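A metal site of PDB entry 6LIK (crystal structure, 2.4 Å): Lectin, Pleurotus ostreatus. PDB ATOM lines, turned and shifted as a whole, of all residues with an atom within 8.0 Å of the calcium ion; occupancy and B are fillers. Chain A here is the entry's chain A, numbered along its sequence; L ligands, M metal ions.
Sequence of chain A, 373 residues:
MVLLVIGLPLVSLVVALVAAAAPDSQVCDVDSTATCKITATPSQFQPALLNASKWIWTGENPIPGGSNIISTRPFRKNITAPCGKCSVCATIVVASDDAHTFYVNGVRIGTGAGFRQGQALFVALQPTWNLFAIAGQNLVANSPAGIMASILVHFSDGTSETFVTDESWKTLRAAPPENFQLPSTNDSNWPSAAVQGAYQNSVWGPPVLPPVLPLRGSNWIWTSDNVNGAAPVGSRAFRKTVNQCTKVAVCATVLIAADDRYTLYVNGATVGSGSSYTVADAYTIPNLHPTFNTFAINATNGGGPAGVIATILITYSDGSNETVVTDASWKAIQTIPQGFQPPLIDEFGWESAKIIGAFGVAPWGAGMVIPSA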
ATOM      1  N   TRP A  57       3.552 -28.211 -16.831  1.00  0.00           N
ATOM      2  CA  TRP A  57       4.293 -27.132 -17.512  1.00  0.00           C
ATOM      3  C   TRP A  57       5.628 -27.768 -17.877  1.00  0.00           C
ATOM      4  O   TRP A  57       5.689 -29.007 -17.886  1.00  0.00           O
ATOM      5  CB  TRP A  57       4.353 -25.886 -16.627  1.00  0.00           C
ATOM      6  CG  TRP A  57       4.702 -24.666 -17.417  1.00  0.00           C
ATOM      7  CD1 TRP A  57       5.860 -23.931 -17.325  1.00  0.00           C
ATOM      8  CD2 TRP A  57       3.922 -24.064 -18.455  1.00  0.00           C
ATOM      9  NE1 TRP A  57       5.837 -22.914 -18.231  1.00  0.00           N
ATOM     10  CE2 TRP A  57       4.678 -22.985 -18.965  1.00  0.00           C
ATOM     11  CE3 TRP A  57       2.672 -24.334 -19.021  1.00  0.00           C
ATOM     12  CZ2 TRP A  57       4.208 -22.147 -19.967  1.00  0.00           C
ATOM     13  CZ3 TRP A  57       2.206 -23.529 -20.040  1.00  0.00           C
ATOM     14  CH2 TRP A  57       2.960 -22.438 -20.497  1.00  0.00           C
ATOM     15  N   GLY A  66       5.654 -22.438  -9.228  1.00  0.00           N
ATOM     16  CA  GLY A  66       6.628 -21.358  -9.054  1.00  0.00           C
ATOM     17  C   GLY A  66       6.501 -20.342 -10.166  1.00  0.00           C
ATOM     18  O   GLY A  66       5.683 -20.564 -11.114  1.00  0.00           O
ATOM     19  N   ASN A  68       7.281 -18.348 -13.433  1.00  0.00           N
ATOM     20  CA  ASN A  68       7.692 -18.662 -14.810  1.00  0.00           C
ATOM     21  C   ASN A  68       7.654 -17.358 -15.616  1.00  0.00           C
ATOM     22  O   ASN A  68       6.937 -16.370 -15.201  1.00  0.00           O
ATOM     23  CB  ASN A  68       6.754 -19.707 -15.398  1.00  0.00           C
ATOM     24  CG  ASN A  68       7.020 -21.061 -14.791  1.00  0.00           C
ATOM     25  OD1 ASN A  68       6.466 -21.401 -13.747  1.00  0.00           O
ATOM     26  ND2 ASN A  68       7.856 -21.846 -15.457  1.00  0.00           N
ATOM     27  N   ILE A  69       8.418 -17.353 -16.692  1.00  0.00           N
ATOM     28  CA  ILE A  69       8.533 -16.216 -17.651  1.00  0.00           C
ATOM     29  C   ILE A  69       7.299 -16.217 -18.560  1.00  0.00           C
ATOM     30  O   ILE A  69       6.696 -17.286 -18.721  1.00  0.00           O
ATOM     31  CB  ILE A  69       9.840 -16.325 -18.464  1.00  0.00           C
ATOM     32  CG1 ILE A  69       9.819 -17.536 -19.407  1.00  0.00           C
ATOM     33  CG2 ILE A  69      11.081 -16.332 -17.557  1.00  0.00           C
ATOM     34  CD1 ILE A  69      11.027 -17.614 -20.319  1.00  0.00           C
ATOM     35  N   ILE A  70       6.996 -15.080 -19.180  1.00  0.00           N
ATOM     36  CA  ILE A  70       6.031 -14.993 -20.319  1.00  0.00           C
ATOM     37  C   ILE A  70       6.585 -15.877 -21.436  1.00  0.00           C
ATOM     38  O   ILE A  70       7.734 -15.727 -21.817  1.00  0.00           O
ATOM     39  CB  ILE A  70       5.791 -13.543 -20.780  1.00  0.00           C
ATOM     40  CG1 ILE A  70       5.103 -12.732 -19.674  1.00  0.00           C
ATOM     41  CG2 ILE A  70       5.006 -13.513 -22.095  1.00  0.00           C
ATOM     42  CD1 ILE A  70       5.095 -11.247 -19.883  1.00  0.00           C
ATOM     43  N   SER A  96      -6.420 -23.546 -17.853  1.00  0.00           N
ATOM     44  CA  SER A  96      -5.063 -23.029 -18.159  1.00  0.00           C
ATOM     45  C   SER A  96      -4.737 -21.812 -17.310  1.00  0.00           C
ATOM     46  O   SER A  96      -5.618 -20.978 -17.020  1.00  0.00           O
ATOM     47  CB  SER A  96      -4.871 -22.758 -19.624  1.00  0.00           C
ATOM     48  OG  SER A  96      -5.840 -21.853 -20.128  1.00  0.00           O
ATOM     49  N   ASP A  97      -3.494 -21.753 -16.901  1.00  0.00           N
ATOM     50  CA  ASP A  97      -2.865 -20.526 -16.400  1.00  0.00           C
ATOM     51  C   ASP A  97      -1.758 -20.190 -17.377  1.00  0.00           C
ATOM     52  O   ASP A  97      -0.695 -20.819 -17.292  1.00  0.00           O
ATOM     53  CB  ASP A  97      -2.379 -20.723 -14.966  1.00  0.00           C
ATOM     54  CG  ASP A  97      -1.778 -19.451 -14.415  1.00  0.00           C
ATOM     55  OD1 ASP A  97      -1.523 -18.534 -15.238  1.00  0.00           O
ATOM     56  OD2 ASP A  97      -1.578 -19.391 -13.190  1.00  0.00           O
ATOM     57  N   ASP A  98      -1.967 -19.246 -18.321  1.00  0.00           N
ATOM     58  CA  ASP A  98      -3.091 -18.329 -18.425  1.00  0.00           C
ATOM     59  C   ASP A  98      -4.016 -18.701 -19.583  1.00  0.00           C
ATOM     60  O   ASP A  98      -5.210 -18.346 -19.510  1.00  0.00           O
ATOM     61  CB  ASP A  98      -2.618 -16.892 -18.700  1.00  0.00           C
ATOM     62  CG  ASP A  98      -1.827 -16.286 -17.543  1.00  0.00           C
ATOM     63  OD1 ASP A  98      -2.487 -15.739 -16.646  1.00  0.00           O
ATOM     64  OD2 ASP A  98      -0.575 -16.441 -17.505  1.00  0.00           O
ATOM     65  N   ALA A  99      -3.520 -19.338 -20.644  1.00  0.00           N
ATOM     66  CA  ALA A  99      -4.362 -19.590 -21.840  1.00  0.00           C
ATOM     67  C   ALA A  99      -3.899 -20.824 -22.612  1.00  0.00           C
ATOM     68  O   ALA A  99      -2.743 -21.262 -22.421  1.00  0.00           O
ATOM     69  CB  ALA A  99      -4.357 -18.360 -22.743  1.00  0.00           C
ATOM     70  N   PHE A 115      -8.177 -20.729 -15.036  1.00  0.00           N
ATOM     71  CA  PHE A 115      -8.006 -21.886 -14.135  1.00  0.00           C
ATOM     72  C   PHE A 115      -9.153 -21.993 -13.126  1.00  0.00           C
ATOM     73  O   PHE A 115      -9.216 -23.041 -12.523  1.00  0.00           O
ATOM     74  CB  PHE A 115      -6.658 -21.819 -13.427  1.00  0.00           C
ATOM     75  CG  PHE A 115      -6.405 -20.575 -12.619  1.00  0.00           C
ATOM     76  CD1 PHE A 115      -6.865 -20.476 -11.315  1.00  0.00           C
ATOM     77  CD2 PHE A 115      -5.674 -19.511 -13.160  1.00  0.00           C
ATOM     78  CE1 PHE A 115      -6.631 -19.328 -10.572  1.00  0.00           C
ATOM     79  CE2 PHE A 115      -5.426 -18.366 -12.408  1.00  0.00           C
ATOM     80  CZ  PHE A 115      -5.924 -18.266 -11.132  1.00  0.00           C
ATOM     81  N   GLN A 137       0.130 -20.834 -22.740  1.00  0.00           N
ATOM     82  CA  GLN A 137       0.799 -19.514 -22.653  1.00  0.00           C
ATOM     83  C   GLN A 137       0.717 -19.035 -21.214  1.00  0.00           C
ATOM     84  O   GLN A 137      -0.390 -19.002 -20.653  1.00  0.00           O
ATOM     85  CB  GLN A 137       0.175 -18.443 -23.554  1.00  0.00           C
ATOM     86  CG  GLN A 137      -0.110 -18.864 -24.995  1.00  0.00           C
ATOM     87  CD  GLN A 137      -0.841 -17.772 -25.751  1.00  0.00           C
ATOM     88  OE1 GLN A 137      -0.542 -16.597 -25.568  1.00  0.00           O
ATOM     89  NE2 GLN A 137      -1.828 -18.143 -26.579  1.00  0.00           N
ATOM     90  N   ASN A 138       1.865 -18.661 -20.663  1.00  0.00           N
ATOM     91  CA  ASN A 138       1.986 -17.784 -19.478  1.00  0.00           C
ATOM     92  C   ASN A 138       2.035 -16.329 -19.971  1.00  0.00           C
ATOM     93  O   ASN A 138       2.901 -16.029 -20.834  1.00  0.00           O
ATOM     94  CB  ASN A 138       3.245 -18.126 -18.680  1.00  0.00           C
ATOM     95  CG  ASN A 138       3.215 -17.533 -17.307  1.00  0.00           C
ATOM     96  OD1 ASN A 138       2.118 -17.328 -16.748  1.00  0.00           O
ATOM     97  ND2 ASN A 138       4.405 -17.255 -16.765  1.00  0.00           N
ATOM     98  N   LEU A 139       1.147 -15.489 -19.445  1.00  0.00           N
ATOM     99  CA  LEU A 139       0.924 -14.086 -19.925  1.00  0.00           C
ATOM    100  C   LEU A 139       1.299 -13.099 -18.834  1.00  0.00           C
ATOM    101  O   LEU A 139       1.273 -11.970 -19.141  1.00  0.00           O
ATOM    102  CB  LEU A 139      -0.537 -13.875 -20.344  1.00  0.00           C
ATOM    103  CG  LEU A 139      -0.998 -14.676 -21.570  1.00  0.00           C
ATOM    104  CD1 LEU A 139      -2.463 -14.437 -21.892  1.00  0.00           C
ATOM    105  CD2 LEU A 139      -0.122 -14.390 -22.792  1.00  0.00           C
ATOM    106  N   VAL A 140       1.633 -13.503 -17.606  1.00  0.00           N
ATOM    107  CA  VAL A 140       2.054 -12.536 -16.542  1.00  0.00           C
ATOM    108  C   VAL A 140       3.461 -12.919 -16.057  1.00  0.00           C
ATOM    109  O   VAL A 140       3.667 -14.084 -15.617  1.00  0.00           O
ATOM    110  CB  VAL A 140       1.033 -12.538 -15.404  1.00  0.00           C
ATOM    111  CG1 VAL A 140       1.457 -11.675 -14.235  1.00  0.00           C
ATOM    112  CG2 VAL A 140      -0.332 -12.141 -15.910  1.00  0.00           C
ATOM    113  N   ALA A 141       4.402 -11.996 -16.140  1.00  0.00           N
ATOM    114  CA  ALA A 141       5.785 -12.199 -15.643  1.00  0.00           C
ATOM    115  C   ALA A 141       5.765 -12.670 -14.184  1.00  0.00           C
ATOM    116  O   ALA A 141       4.934 -12.175 -13.415  1.00  0.00           O
ATOM    117  CB  ALA A 141       6.567 -10.918 -15.775  1.00  0.00           C
ATOM    118  N   ASN A 142       6.685 -13.582 -13.830  1.00  0.00           N
ATOM    119  CA  ASN A 142       6.894 -14.038 -12.438  1.00  0.00           C
ATOM    120  C   ASN A 142       5.661 -14.765 -11.872  1.00  0.00           C
ATOM    121  O   ASN A 142       5.500 -14.809 -10.626  1.00  0.00           O
ATOM    122  CB  ASN A 142       7.258 -12.887 -11.511  1.00  0.00           C
ATOM    123  CG  ASN A 142       8.471 -12.142 -12.002  1.00  0.00           C
ATOM    124  OD1 ASN A 142       9.451 -12.763 -12.376  1.00  0.00           O
ATOM    125  ND2 ASN A 142       8.370 -10.834 -12.090  1.00  0.00           N
ATOM    126  N   SER A 143       4.827 -15.327 -12.744  1.00  0.00           N
ATOM    127  CA  SER A 143       3.567 -15.951 -12.311  1.00  0.00           C
ATOM    128  C   SER A 143       3.631 -17.449 -12.587  1.00  0.00           C
ATOM    129  O   SER A 143       4.360 -17.925 -13.466  1.00  0.00           O
ATOM    130  CB  SER A 143       2.377 -15.284 -12.969  1.00  0.00           C
ATOM    131  OG  SER A 143       2.265 -15.699 -14.311  1.00  0.00           O
ATOM    132  N   PRO A 144       2.801 -18.228 -11.848  1.00  0.00           N
ATOM    133  CA  PRO A 144       2.672 -19.642 -12.104  1.00  0.00           C
ATOM    134  C   PRO A 144       2.158 -19.890 -13.529  1.00  0.00           C
ATOM    135  O   PRO A 144       1.614 -19.013 -14.112  1.00  0.00           O
ATOM    136  CB  PRO A 144       1.670 -20.165 -11.085  1.00  0.00           C
ATOM    137  CG  PRO A 144       1.302 -19.018 -10.224  1.00  0.00           C
ATOM    138  CD  PRO A 144       1.954 -17.769 -10.758  1.00  0.00           C
ATOM    139  N   ALA A 145       2.425 -21.066 -14.072  1.00  0.00           N
ATOM    140  CA  ALA A 145       1.972 -21.484 -15.408  1.00  0.00           C
ATOM    141  C   ALA A 145       1.586 -22.971 -15.392  1.00  0.00           C
ATOM    142  O   ALA A 145       2.208 -23.768 -14.629  1.00  0.00           O
ATOM    143  CB  ALA A 145       3.039 -21.191 -16.409  1.00  0.00           C
ATOM    144  N   GLY A 146       0.542 -23.329 -16.142  1.00  0.00           N
ATOM    145  CA  GLY A 146       0.084 -24.718 -16.124  1.00  0.00           C
ATOM    146  C   GLY A 146      -1.113 -24.980 -16.988  1.00  0.00           C
ATOM    147  O   GLY A 146      -1.912 -24.099 -17.164  1.00  0.00           O
ATOM    148  N   TRP A 204      -3.481 -23.424  -7.733  1.00  0.00           N
ATOM    149  CA  TRP A 204      -4.743 -23.012  -8.378  1.00  0.00           C
ATOM    150  C   TRP A 204      -5.964 -23.434  -7.569  1.00  0.00           C
ATOM    151  O   TRP A 204      -6.948 -22.797  -7.740  1.00  0.00           O
ATOM    152  CB  TRP A 204      -4.800 -23.545  -9.815  1.00  0.00           C
ATOM    153  CG  TRP A 204      -3.689 -22.966 -10.610  1.00  0.00           C
ATOM    154  CD1 TRP A 204      -3.561 -21.683 -11.056  1.00  0.00           C
ATOM    155  CD2 TRP A 204      -2.485 -23.649 -10.972  1.00  0.00           C
ATOM    156  NE1 TRP A 204      -2.374 -21.541 -11.717  1.00  0.00           N
ATOM    157  CE2 TRP A 204      -1.692 -22.722 -11.673  1.00  0.00           C
ATOM    158  CE3 TRP A 204      -2.001 -24.936 -10.758  1.00  0.00           C
ATOM    159  CZ2 TRP A 204      -0.427 -23.052 -12.164  1.00  0.00           C
ATOM    160  CZ3 TRP A 204      -0.762 -25.267 -11.227  1.00  0.00           C
ATOM    161  CH2 TRP A 204       0.010 -24.330 -11.935  1.00  0.00           C
HETATM  162  C1  LIG L   1      -1.974 -16.176 -11.187  1.00  0.00           C
HETATM  163  O1  LIG L   1      -2.988 -15.195 -10.983  1.00  0.00           O
HETATM  164  C2  LIG L   1      -1.632 -16.327 -12.653  1.00  0.00           C
HETATM  165  O2  LIG L   1      -0.377 -16.971 -12.880  1.00  0.00           O
HETATM  166  C3  LIG L   1      -1.640 -15.003 -13.377  1.00  0.00           C
HETATM  167  O3  LIG L   1      -1.047 -15.150 -14.669  1.00  0.00           O
HETATM  168 CA    CA M   1       0.399 -17.148 -15.199  1.00  0.00          CA
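The side-chain amide nitrogen (ND2) of Asn 138 sits at hydrogen-bond distance from the backbone carbonyl oxygen (O) of Val 140, at 3.5 Å.
The side-chain amide nitrogen (ND2) of Asn 138 is in hydrogen-bond range of the backbone carbonyl oxygen (O) of Asn 68 (3.1 Å).
O of Ile 69 lies within hydrogen-bond range of ND2 of Asn 138, 3.0 Å away.
NE1 of Trp 204 is in hydrogen-bond range of OD2 of Asp 97, at 2.7 Å.
The backbone NH (N) of Asp 97 lies within hydrogen-bond range of the backbone carbonyl oxygen (O) of Gly 146.
The backbone carbonyl oxygen of Val 140 sits close to the side-chain hydroxyl of Ser 143 (2.5 Å).
The backbone NH of Asn 68 sits at hydrogen-bond distance from the backbone carbonyl oxygen of Ser 143, at 3.0 Å.
The backbone NH (N) of Asp 98 is in hydrogen-bond range of the backbone carbonyl oxygen (O) of Gln 137, at 2.8 Å.
Five residues have an atom within 4 Å of the calcium ion: Asp 97, Asp 98, Asn 138, Ser 143 and Pro 144.
The nearest printed residue that does not touch the calcium ion is Val 140 (4.5 Å).
The calcium ion is bound by OD1 of Asn 138 (2.3 Å), OD1 of Asp 97 (2.4 Å), O2 of the ligand (2.5 Å), O of Pro 144 (2.5 Å), O3 of the ligand (2.5 Å), OG of Ser 143 (2.5 Å) and OD2 of Asp 98 (2.6 Å).
The calcium ion has seven donor atoms within binding distance.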
